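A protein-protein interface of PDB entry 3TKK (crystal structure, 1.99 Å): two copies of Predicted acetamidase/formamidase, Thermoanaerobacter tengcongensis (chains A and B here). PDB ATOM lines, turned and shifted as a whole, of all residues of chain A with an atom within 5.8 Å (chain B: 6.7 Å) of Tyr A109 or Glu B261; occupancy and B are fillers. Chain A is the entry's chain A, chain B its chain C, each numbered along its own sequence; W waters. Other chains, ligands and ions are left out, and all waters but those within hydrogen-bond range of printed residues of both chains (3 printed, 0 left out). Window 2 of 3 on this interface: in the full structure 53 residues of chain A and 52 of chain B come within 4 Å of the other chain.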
ATOM      1  N   LEU A  51     -15.835 -12.053  17.964  1.00  0.00           N
ATOM      2  CA  LEU A  51     -15.250 -11.397  19.124  1.00  0.00           C
ATOM      3  C   LEU A  51     -15.174 -12.369  20.312  1.00  0.00           C
ATOM      4  O   LEU A  51     -15.824 -13.432  20.318  1.00  0.00           O
ATOM      5  CB  LEU A  51     -16.011 -10.100  19.501  1.00  0.00           C
ATOM      6  CG  LEU A  51     -15.310  -9.141  20.502  1.00  0.00           C
ATOM      7  CD1 LEU A  51     -13.764  -9.283  20.465  1.00  0.00           C
ATOM      8  CD2 LEU A  51     -15.760  -7.650  20.345  1.00  0.00           C
ATOM      9  N   ASP A  52     -14.342 -11.997  21.292  1.00  0.00           N
ATOM     10  CA  ASP A  52     -14.146 -12.789  22.519  1.00  0.00           C
ATOM     11  C   ASP A  52     -15.467 -13.025  23.300  1.00  0.00           C
ATOM     12  O   ASP A  52     -15.812 -12.310  24.259  1.00  0.00           O
ATOM     13  CB  ASP A  52     -13.017 -12.195  23.405  1.00  0.00           C
ATOM     14  CG  ASP A  52     -11.620 -12.271  22.727  1.00  0.00           C
ATOM     15  OD1 ASP A  52     -11.313 -11.371  21.909  1.00  0.00           O
ATOM     16  OD2 ASP A  52     -10.834 -13.223  23.010  1.00  0.00           O
ATOM     17  N   LEU A  92      -4.821 -10.736  17.146  1.00  0.00           N
ATOM     18  CA  LEU A  92      -4.254  -9.962  18.206  1.00  0.00           C
ATOM     19  C   LEU A  92      -5.451  -9.734  19.127  1.00  0.00           C
ATOM     20  O   LEU A  92      -6.578  -9.419  18.610  1.00  0.00           O
ATOM     21  CB  LEU A  92      -3.784  -8.582  17.677  1.00  0.00           C
ATOM     22  CG  LEU A  92      -2.559  -8.866  16.842  1.00  0.00           C
ATOM     23  CD1 LEU A  92      -2.274  -7.752  15.935  1.00  0.00           C
ATOM     24  CD2 LEU A  92      -1.437  -9.062  17.893  1.00  0.00           C
ATOM     25  N   ALA A  93      -5.210  -9.827  20.433  1.00  0.00           N
ATOM     26  CA  ALA A  93      -6.200  -9.594  21.491  1.00  0.00           C
ATOM     27  C   ALA A  93      -5.680  -8.740  22.589  1.00  0.00           C
ATOM     28  O   ALA A  93      -4.495  -8.848  22.999  1.00  0.00           O
ATOM     29  CB  ALA A  93      -6.732 -10.958  22.050  1.00  0.00           C
ATOM     30  N   THR A  94      -6.549  -7.841  23.111  1.00  0.00           N
ATOM     31  CA  THR A  94      -6.210  -7.205  24.392  1.00  0.00           C
ATOM     32  C   THR A  94      -7.483  -6.683  25.005  1.00  0.00           C
ATOM     33  O   THR A  94      -8.517  -7.011  24.538  1.00  0.00           O
ATOM     34  CB  THR A  94      -5.272  -5.996  24.189  1.00  0.00           C
ATOM     35  OG1 THR A  94      -4.769  -5.542  25.461  1.00  0.00           O
ATOM     36  CG2 THR A  94      -5.960  -4.816  23.426  1.00  0.00           C
ATOM     37  N   GLY A  95      -7.417  -5.825  26.014  1.00  0.00           N
ATOM     38  CA  GLY A  95      -8.677  -5.273  26.528  1.00  0.00           C
ATOM     39  C   GLY A  95      -8.694  -4.966  27.994  1.00  0.00           C
ATOM     40  O   GLY A  95      -7.658  -5.064  28.640  1.00  0.00           O
ATOM     41  N   LEU A  98      -6.586  -6.650  30.780  1.00  0.00           N
ATOM     42  CA  LEU A  98      -5.675  -7.677  30.212  1.00  0.00           C
ATOM     43  C   LEU A  98      -4.268  -7.139  29.987  1.00  0.00           C
ATOM     44  O   LEU A  98      -4.142  -6.136  29.378  1.00  0.00           O
ATOM     45  CB  LEU A  98      -6.219  -8.278  28.913  1.00  0.00           C
ATOM     46  CG  LEU A  98      -7.691  -8.871  28.932  1.00  0.00           C
ATOM     47  CD1 LEU A  98      -8.293  -9.148  27.475  1.00  0.00           C
ATOM     48  CD2 LEU A  98      -7.864 -10.129  29.892  1.00  0.00           C
ATOM     49  N   MET A 105      -8.047   0.308  29.389  1.00  0.00           N
ATOM     50  CA  MET A 105      -8.930  -0.059  28.294  1.00  0.00           C
ATOM     51  C   MET A 105     -10.289  -0.477  28.846  1.00  0.00           C
ATOM     52  O   MET A 105     -10.351  -0.851  29.979  1.00  0.00           O
ATOM     53  CB  MET A 105      -8.310  -1.241  27.537  1.00  0.00           C
ATOM     54  CG  MET A 105      -7.176  -0.731  26.545  1.00  0.00           C
ATOM     55  SD  MET A 105      -6.407  -2.082  25.734  1.00  0.00           S
ATOM     56  CE  MET A 105      -5.306  -2.761  27.011  1.00  0.00           C
ATOM     57  N   GLU A 106     -11.326  -0.435  28.007  1.00  0.00           N
ATOM     58  CA  GLU A 106     -12.709  -0.806  28.376  1.00  0.00           C
ATOM     59  C   GLU A 106     -13.155  -1.900  27.399  1.00  0.00           C
ATOM     60  O   GLU A 106     -12.731  -1.901  26.231  1.00  0.00           O
ATOM     61  CB  GLU A 106     -13.580   0.398  28.207  1.00  0.00           C
ATOM     62  CG  GLU A 106     -13.293   1.483  29.231  1.00  0.00           C
ATOM     63  CD  GLU A 106     -13.544   0.979  30.645  1.00  0.00           C
ATOM     64  OE1 GLU A 106     -14.209  -0.068  30.830  1.00  0.00           O
ATOM     65  OE2 GLU A 106     -13.076   1.655  31.582  1.00  0.00           O
ATOM     66  N   GLY A 107     -13.961  -2.859  27.846  1.00  0.00           N
ATOM     67  CA  GLY A 107     -14.321  -3.968  26.971  1.00  0.00           C
ATOM     68  C   GLY A 107     -13.166  -4.858  26.476  1.00  0.00           C
ATOM     69  O   GLY A 107     -12.120  -4.990  27.128  1.00  0.00           O
ATOM     70  N   LEU A 108     -13.377  -5.521  25.340  1.00  0.00           N
ATOM     71  CA  LEU A 108     -12.498  -6.572  24.907  1.00  0.00           C
ATOM     72  C   LEU A 108     -12.146  -6.315  23.420  1.00  0.00           C
ATOM     73  O   LEU A 108     -12.986  -5.916  22.653  1.00  0.00           O
ATOM     74  CB  LEU A 108     -13.210  -7.937  25.044  1.00  0.00           C
ATOM     75  CG  LEU A 108     -12.252  -9.084  25.422  1.00  0.00           C
ATOM     76  CD1 LEU A 108     -10.893  -9.218  24.560  1.00  0.00           C
ATOM     77  CD2 LEU A 108     -11.878  -8.937  26.936  1.00  0.00           C
ATOM     78  N   TYR A 109     -10.912  -6.568  23.016  1.00  0.00           N
ATOM     79  CA  TYR A 109     -10.512  -6.184  21.683  1.00  0.00           C
ATOM     80  C   TYR A 109      -9.950  -7.389  21.042  1.00  0.00           C
ATOM     81  O   TYR A 109      -9.302  -8.154  21.733  1.00  0.00           O
ATOM     82  CB  TYR A 109      -9.357  -5.190  21.772  1.00  0.00           C
ATOM     83  CG  TYR A 109      -8.714  -4.788  20.442  1.00  0.00           C
ATOM     84  CD1 TYR A 109      -9.244  -3.772  19.666  1.00  0.00           C
ATOM     85  CD2 TYR A 109      -7.556  -5.416  19.985  1.00  0.00           C
ATOM     86  CE1 TYR A 109      -8.644  -3.365  18.430  1.00  0.00           C
ATOM     87  CE2 TYR A 109      -6.931  -5.001  18.757  1.00  0.00           C
ATOM     88  CZ  TYR A 109      -7.483  -3.960  18.031  1.00  0.00           C
ATOM     89  OH  TYR A 109      -6.850  -3.565  16.877  1.00  0.00           O
ATOM     90  N   SER A 110     -10.235  -7.579  19.747  1.00  0.00           N
ATOM     91  CA  SER A 110      -9.395  -8.454  18.904  1.00  0.00           C
ATOM     92  C   SER A 110      -9.300  -7.902  17.496  1.00  0.00           C
ATOM     93  O   SER A 110     -10.181  -7.185  17.039  1.00  0.00           O
ATOM     94  CB  SER A 110      -9.973  -9.865  18.780  1.00  0.00           C
ATOM     95  OG  SER A 110     -11.239  -9.811  18.162  1.00  0.00           O
ATOM     96  N   LYS A 111      -8.218  -8.240  16.796  1.00  0.00           N
ATOM     97  CA  LYS A 111      -8.041  -7.837  15.434  1.00  0.00           C
ATOM     98  C   LYS A 111      -7.458  -9.006  14.699  1.00  0.00           C
ATOM     99  O   LYS A 111      -6.390  -9.546  15.109  1.00  0.00           O
ATOM    100  CB  LYS A 111      -6.981  -6.760  15.352  1.00  0.00           C
ATOM    101  CG  LYS A 111      -6.842  -6.179  13.924  1.00  0.00           C
ATOM    102  CD  LYS A 111      -5.820  -5.087  13.997  1.00  0.00           C
ATOM    103  CE  LYS A 111      -6.286  -4.053  13.009  1.00  0.00           C
ATOM    104  NZ  LYS A 111      -6.922  -4.796  11.847  1.00  0.00           N
ATOM    105  N   PHE A 122       0.180  -5.530  10.368  1.00  0.00           N
ATOM    106  CA  PHE A 122      -0.410  -4.983  11.611  1.00  0.00           C
ATOM    107  C   PHE A 122      -1.435  -3.911  11.245  1.00  0.00           C
ATOM    108  O   PHE A 122      -2.538  -3.833  11.838  1.00  0.00           O
ATOM    109  CB  PHE A 122       0.730  -4.407  12.504  1.00  0.00           C
ATOM    110  CG  PHE A 122       0.271  -3.819  13.801  1.00  0.00           C
ATOM    111  CD1 PHE A 122      -0.056  -4.641  14.863  1.00  0.00           C
ATOM    112  CD2 PHE A 122       0.012  -2.455  13.888  1.00  0.00           C
ATOM    113  CE1 PHE A 122      -0.489  -4.102  16.108  1.00  0.00           C
ATOM    114  CE2 PHE A 122      -0.441  -1.892  15.031  1.00  0.00           C
ATOM    115  CZ  PHE A 122      -0.693  -2.728  16.181  1.00  0.00           C
ATOM    116  N   LEU B 258      -2.377   6.693  17.635  1.00  0.00           N
ATOM    117  CA  LEU B 258      -2.659   5.247  17.752  1.00  0.00           C
ATOM    118  C   LEU B 258      -3.588   5.009  18.938  1.00  0.00           C
ATOM    119  O   LEU B 258      -3.345   5.560  20.042  1.00  0.00           O
ATOM    120  CB  LEU B 258      -1.342   4.526  17.975  1.00  0.00           C
ATOM    121  CG  LEU B 258      -1.081   3.088  17.524  1.00  0.00           C
ATOM    122  CD1 LEU B 258      -0.015   2.284  18.228  1.00  0.00           C
ATOM    123  CD2 LEU B 258      -2.127   2.404  16.797  1.00  0.00           C
ATOM    124  N   SER B 259      -4.628   4.226  18.738  1.00  0.00           N
ATOM    125  CA  SER B 259      -5.540   3.898  19.841  1.00  0.00           C
ATOM    126  C   SER B 259      -4.901   3.093  20.966  1.00  0.00           C
ATOM    127  O   SER B 259      -3.871   2.478  20.822  1.00  0.00           O
ATOM    128  CB  SER B 259      -6.742   3.124  19.336  1.00  0.00           C
ATOM    129  OG  SER B 259      -6.359   1.762  19.057  1.00  0.00           O
ATOM    130  N   THR B 260      -5.528   3.074  22.142  1.00  0.00           N
ATOM    131  CA  THR B 260      -4.886   2.392  23.259  1.00  0.00           C
ATOM    132  C   THR B 260      -4.687   0.917  22.886  1.00  0.00           C
ATOM    133  O   THR B 260      -3.642   0.305  23.257  1.00  0.00           O
ATOM    134  CB  THR B 260      -5.853   2.492  24.528  1.00  0.00           C
ATOM    135  OG1 THR B 260      -6.271   3.879  24.647  1.00  0.00           O
ATOM    136  CG2 THR B 260      -5.085   2.069  25.749  1.00  0.00           C
ATOM    137  N   GLU B 261      -5.712   0.335  22.243  1.00  0.00           N
ATOM    138  CA  GLU B 261      -5.706  -1.074  21.874  1.00  0.00           C
ATOM    139  C   GLU B 261      -4.570  -1.288  20.862  1.00  0.00           C
ATOM    140  O   GLU B 261      -3.871  -2.302  20.894  1.00  0.00           O
ATOM    141  CB  GLU B 261      -7.049  -1.498  21.243  1.00  0.00           C
ATOM    142  CG  GLU B 261      -8.231  -1.665  22.293  1.00  0.00           C
ATOM    143  CD  GLU B 261      -8.721  -0.303  22.723  1.00  0.00           C
ATOM    144  OE1 GLU B 261      -8.384   0.810  22.112  1.00  0.00           O
ATOM    145  OE2 GLU B 261      -9.333  -0.310  23.769  1.00  0.00           O
ATOM    146  N   GLY B 262      -4.460  -0.342  19.959  1.00  0.00           N
ATOM    147  CA  GLY B 262      -3.343  -0.256  19.027  1.00  0.00           C
ATOM    148  C   GLY B 262      -2.003  -0.312  19.744  1.00  0.00           C
ATOM    149  O   GLY B 262      -1.076  -1.020  19.353  1.00  0.00           O
ATOM    150  N   ILE B 263      -1.924   0.506  20.762  1.00  0.00           N
ATOM    151  CA  ILE B 263      -0.714   0.578  21.593  1.00  0.00           C
ATOM    152  C   ILE B 263      -0.389  -0.719  22.276  1.00  0.00           C
ATOM    153  O   ILE B 263       0.731  -1.211  22.175  1.00  0.00           O
ATOM    154  CB  ILE B 263      -0.759   1.741  22.528  1.00  0.00           C
ATOM    155  CG1 ILE B 263      -0.664   3.050  21.666  1.00  0.00           C
ATOM    156  CG2 ILE B 263       0.513   1.733  23.452  1.00  0.00           C
ATOM    157  CD1 ILE B 263      -1.182   4.378  22.393  1.00  0.00           C
ATOM    158  N   ALA B 264      -1.383  -1.273  22.951  1.00  0.00           N
ATOM    159  CA  ALA B 264      -1.161  -2.442  23.758  1.00  0.00           C
ATOM    160  C   ALA B 264      -0.742  -3.613  22.865  1.00  0.00           C
ATOM    161  O   ALA B 264       0.277  -4.319  23.166  1.00  0.00           O
ATOM    162  CB  ALA B 264      -2.471  -2.792  24.525  1.00  0.00           C
ATOM    163  N   THR B 265      -1.435  -3.797  21.742  1.00  0.00           N
ATOM    164  CA  THR B 265      -1.108  -4.933  20.884  1.00  0.00           C
ATOM    165  C   THR B 265       0.247  -4.752  20.108  1.00  0.00           C
ATOM    166  O   THR B 265       1.017  -5.746  19.941  1.00  0.00           O
ATOM    167  CB  THR B 265      -2.282  -5.267  19.842  1.00  0.00           C
ATOM    168  OG1 THR B 265      -2.571  -4.087  19.056  1.00  0.00           O
ATOM    169  CG2 THR B 265      -3.458  -5.687  20.557  1.00  0.00           C
ATOM    170  N   LEU B 266       0.559  -3.521  19.698  1.00  0.00           N
ATOM    171  CA  LEU B 266       1.853  -3.217  19.028  1.00  0.00           C
ATOM    172  C   LEU B 266       3.014  -3.555  20.033  1.00  0.00           C
ATOM    173  O   LEU B 266       3.984  -4.238  19.701  1.00  0.00           O
ATOM    174  CB  LEU B 266       1.989  -1.690  18.629  1.00  0.00           C
ATOM    175  CG  LEU B 266       3.301  -1.340  17.845  1.00  0.00           C
ATOM    176  CD1 LEU B 266       3.348  -2.231  16.619  1.00  0.00           C
ATOM    177  CD2 LEU B 266       3.442   0.233  17.423  1.00  0.00           C
HETATM  178  O   HOH W   1     -10.635  -2.540  24.349  1.00  0.00           O
HETATM  179  O   HOH W   2      -4.049  -4.084  16.675  1.00  0.00           O
HETATM  180  O   HOH W   3     -10.793   1.000  25.715  1.00  0.00           O
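Of the printed residues of chain B, Thr A94 touches Ala B264 and Thr B265. Of chain B, only Glu B261 (3.5 Å) and Thr B265 (3.97 Å) come within 4 Å of Tyr A109. Ser A110 touches none of the printed residues of chain B. Printed residues of chain B within 4 Å of Phe A122: Gly B262, Thr B265 and Leu B266. Printed residues of chain A within 4 Å of Thr B260: Met A105 (3.6 Å). Glu B261 touches just these residues of chain A: Met A105 and Tyr A109. Of the printed residues of chain A, Thr B265 touches Thr A94 (3.9 Å), Tyr A109 (3.97 Å) and Phe A122 (3.6 Å). The nearest printed residue of chain B that does not touch Thr A94 is Glu B261 (4.05 Å).
Printed residues of chain A that touch a printed residue of chain B: Thr A94, Met A105, Tyr A109 and Phe A122. Hydrophobic or aromatic side chains of chain A within 4 Å of the printed part of chain B: Met A105, Tyr A109 and Phe A122. Among the printed residues, no Asp or Glu carboxylate lies within 4 Å of a Lys or Arg side-chain nitrogen of the other chain.
No position is printed for both chains. Of the 10 pairs that touch across the chains among the printed residues, none has its exchanged pair printed and touching as well.
The side-chain hydroxyl of Thr B265 lies within hydrogen-bond range of the backbone carbonyl oxygen of Glu B261. The backbone NH (N) of Gly B262 lies within hydrogen-bond range of the side-chain hydroxyl (OG) of Ser B259, 3.0 Å away. The backbone carbonyl oxygen (O) of Thr A94 sits at hydrogen-bond distance from the backbone NH (N) of Tyr A109 (2.9 Å). The backbone carbonyl oxygen of Gly B262 is in hydrogen-bond range of the side-chain hydroxyl of Thr B265, 3.4 Å away.
Water W1 lies within hydrogen-bond range of OE2 of Glu B261 (2.6 Å) and O of Glu A106 (2.9 Å). Water W3 lies within hydrogen-bond range of N of Glu A106 (2.8 Å) and OE2 of Glu B261 (2.8 Å). Water W2 bridges OG1 of Thr B265 and OH of Tyr A109.
Ala B264 touches Thr A94. Thr A94 touches Thr B265. Met A105 touches Thr B260. Glu B261 touches Met A105 (OE2 to CG, 3.5 Å). Met A105 touches Ala B264. CD1 of Tyr A109 touches CG of Glu B261, at 3.5 Å. Thr B265 touches Tyr A109 (CG2 to CE2, 3.97 Å). Phe A122 touches Gly B262. CE1 of Phe A122 touches OG1 of Thr B265 (3.6 Å). CB of Leu B266 touches CZ of Phe A122 (3.8 Å).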
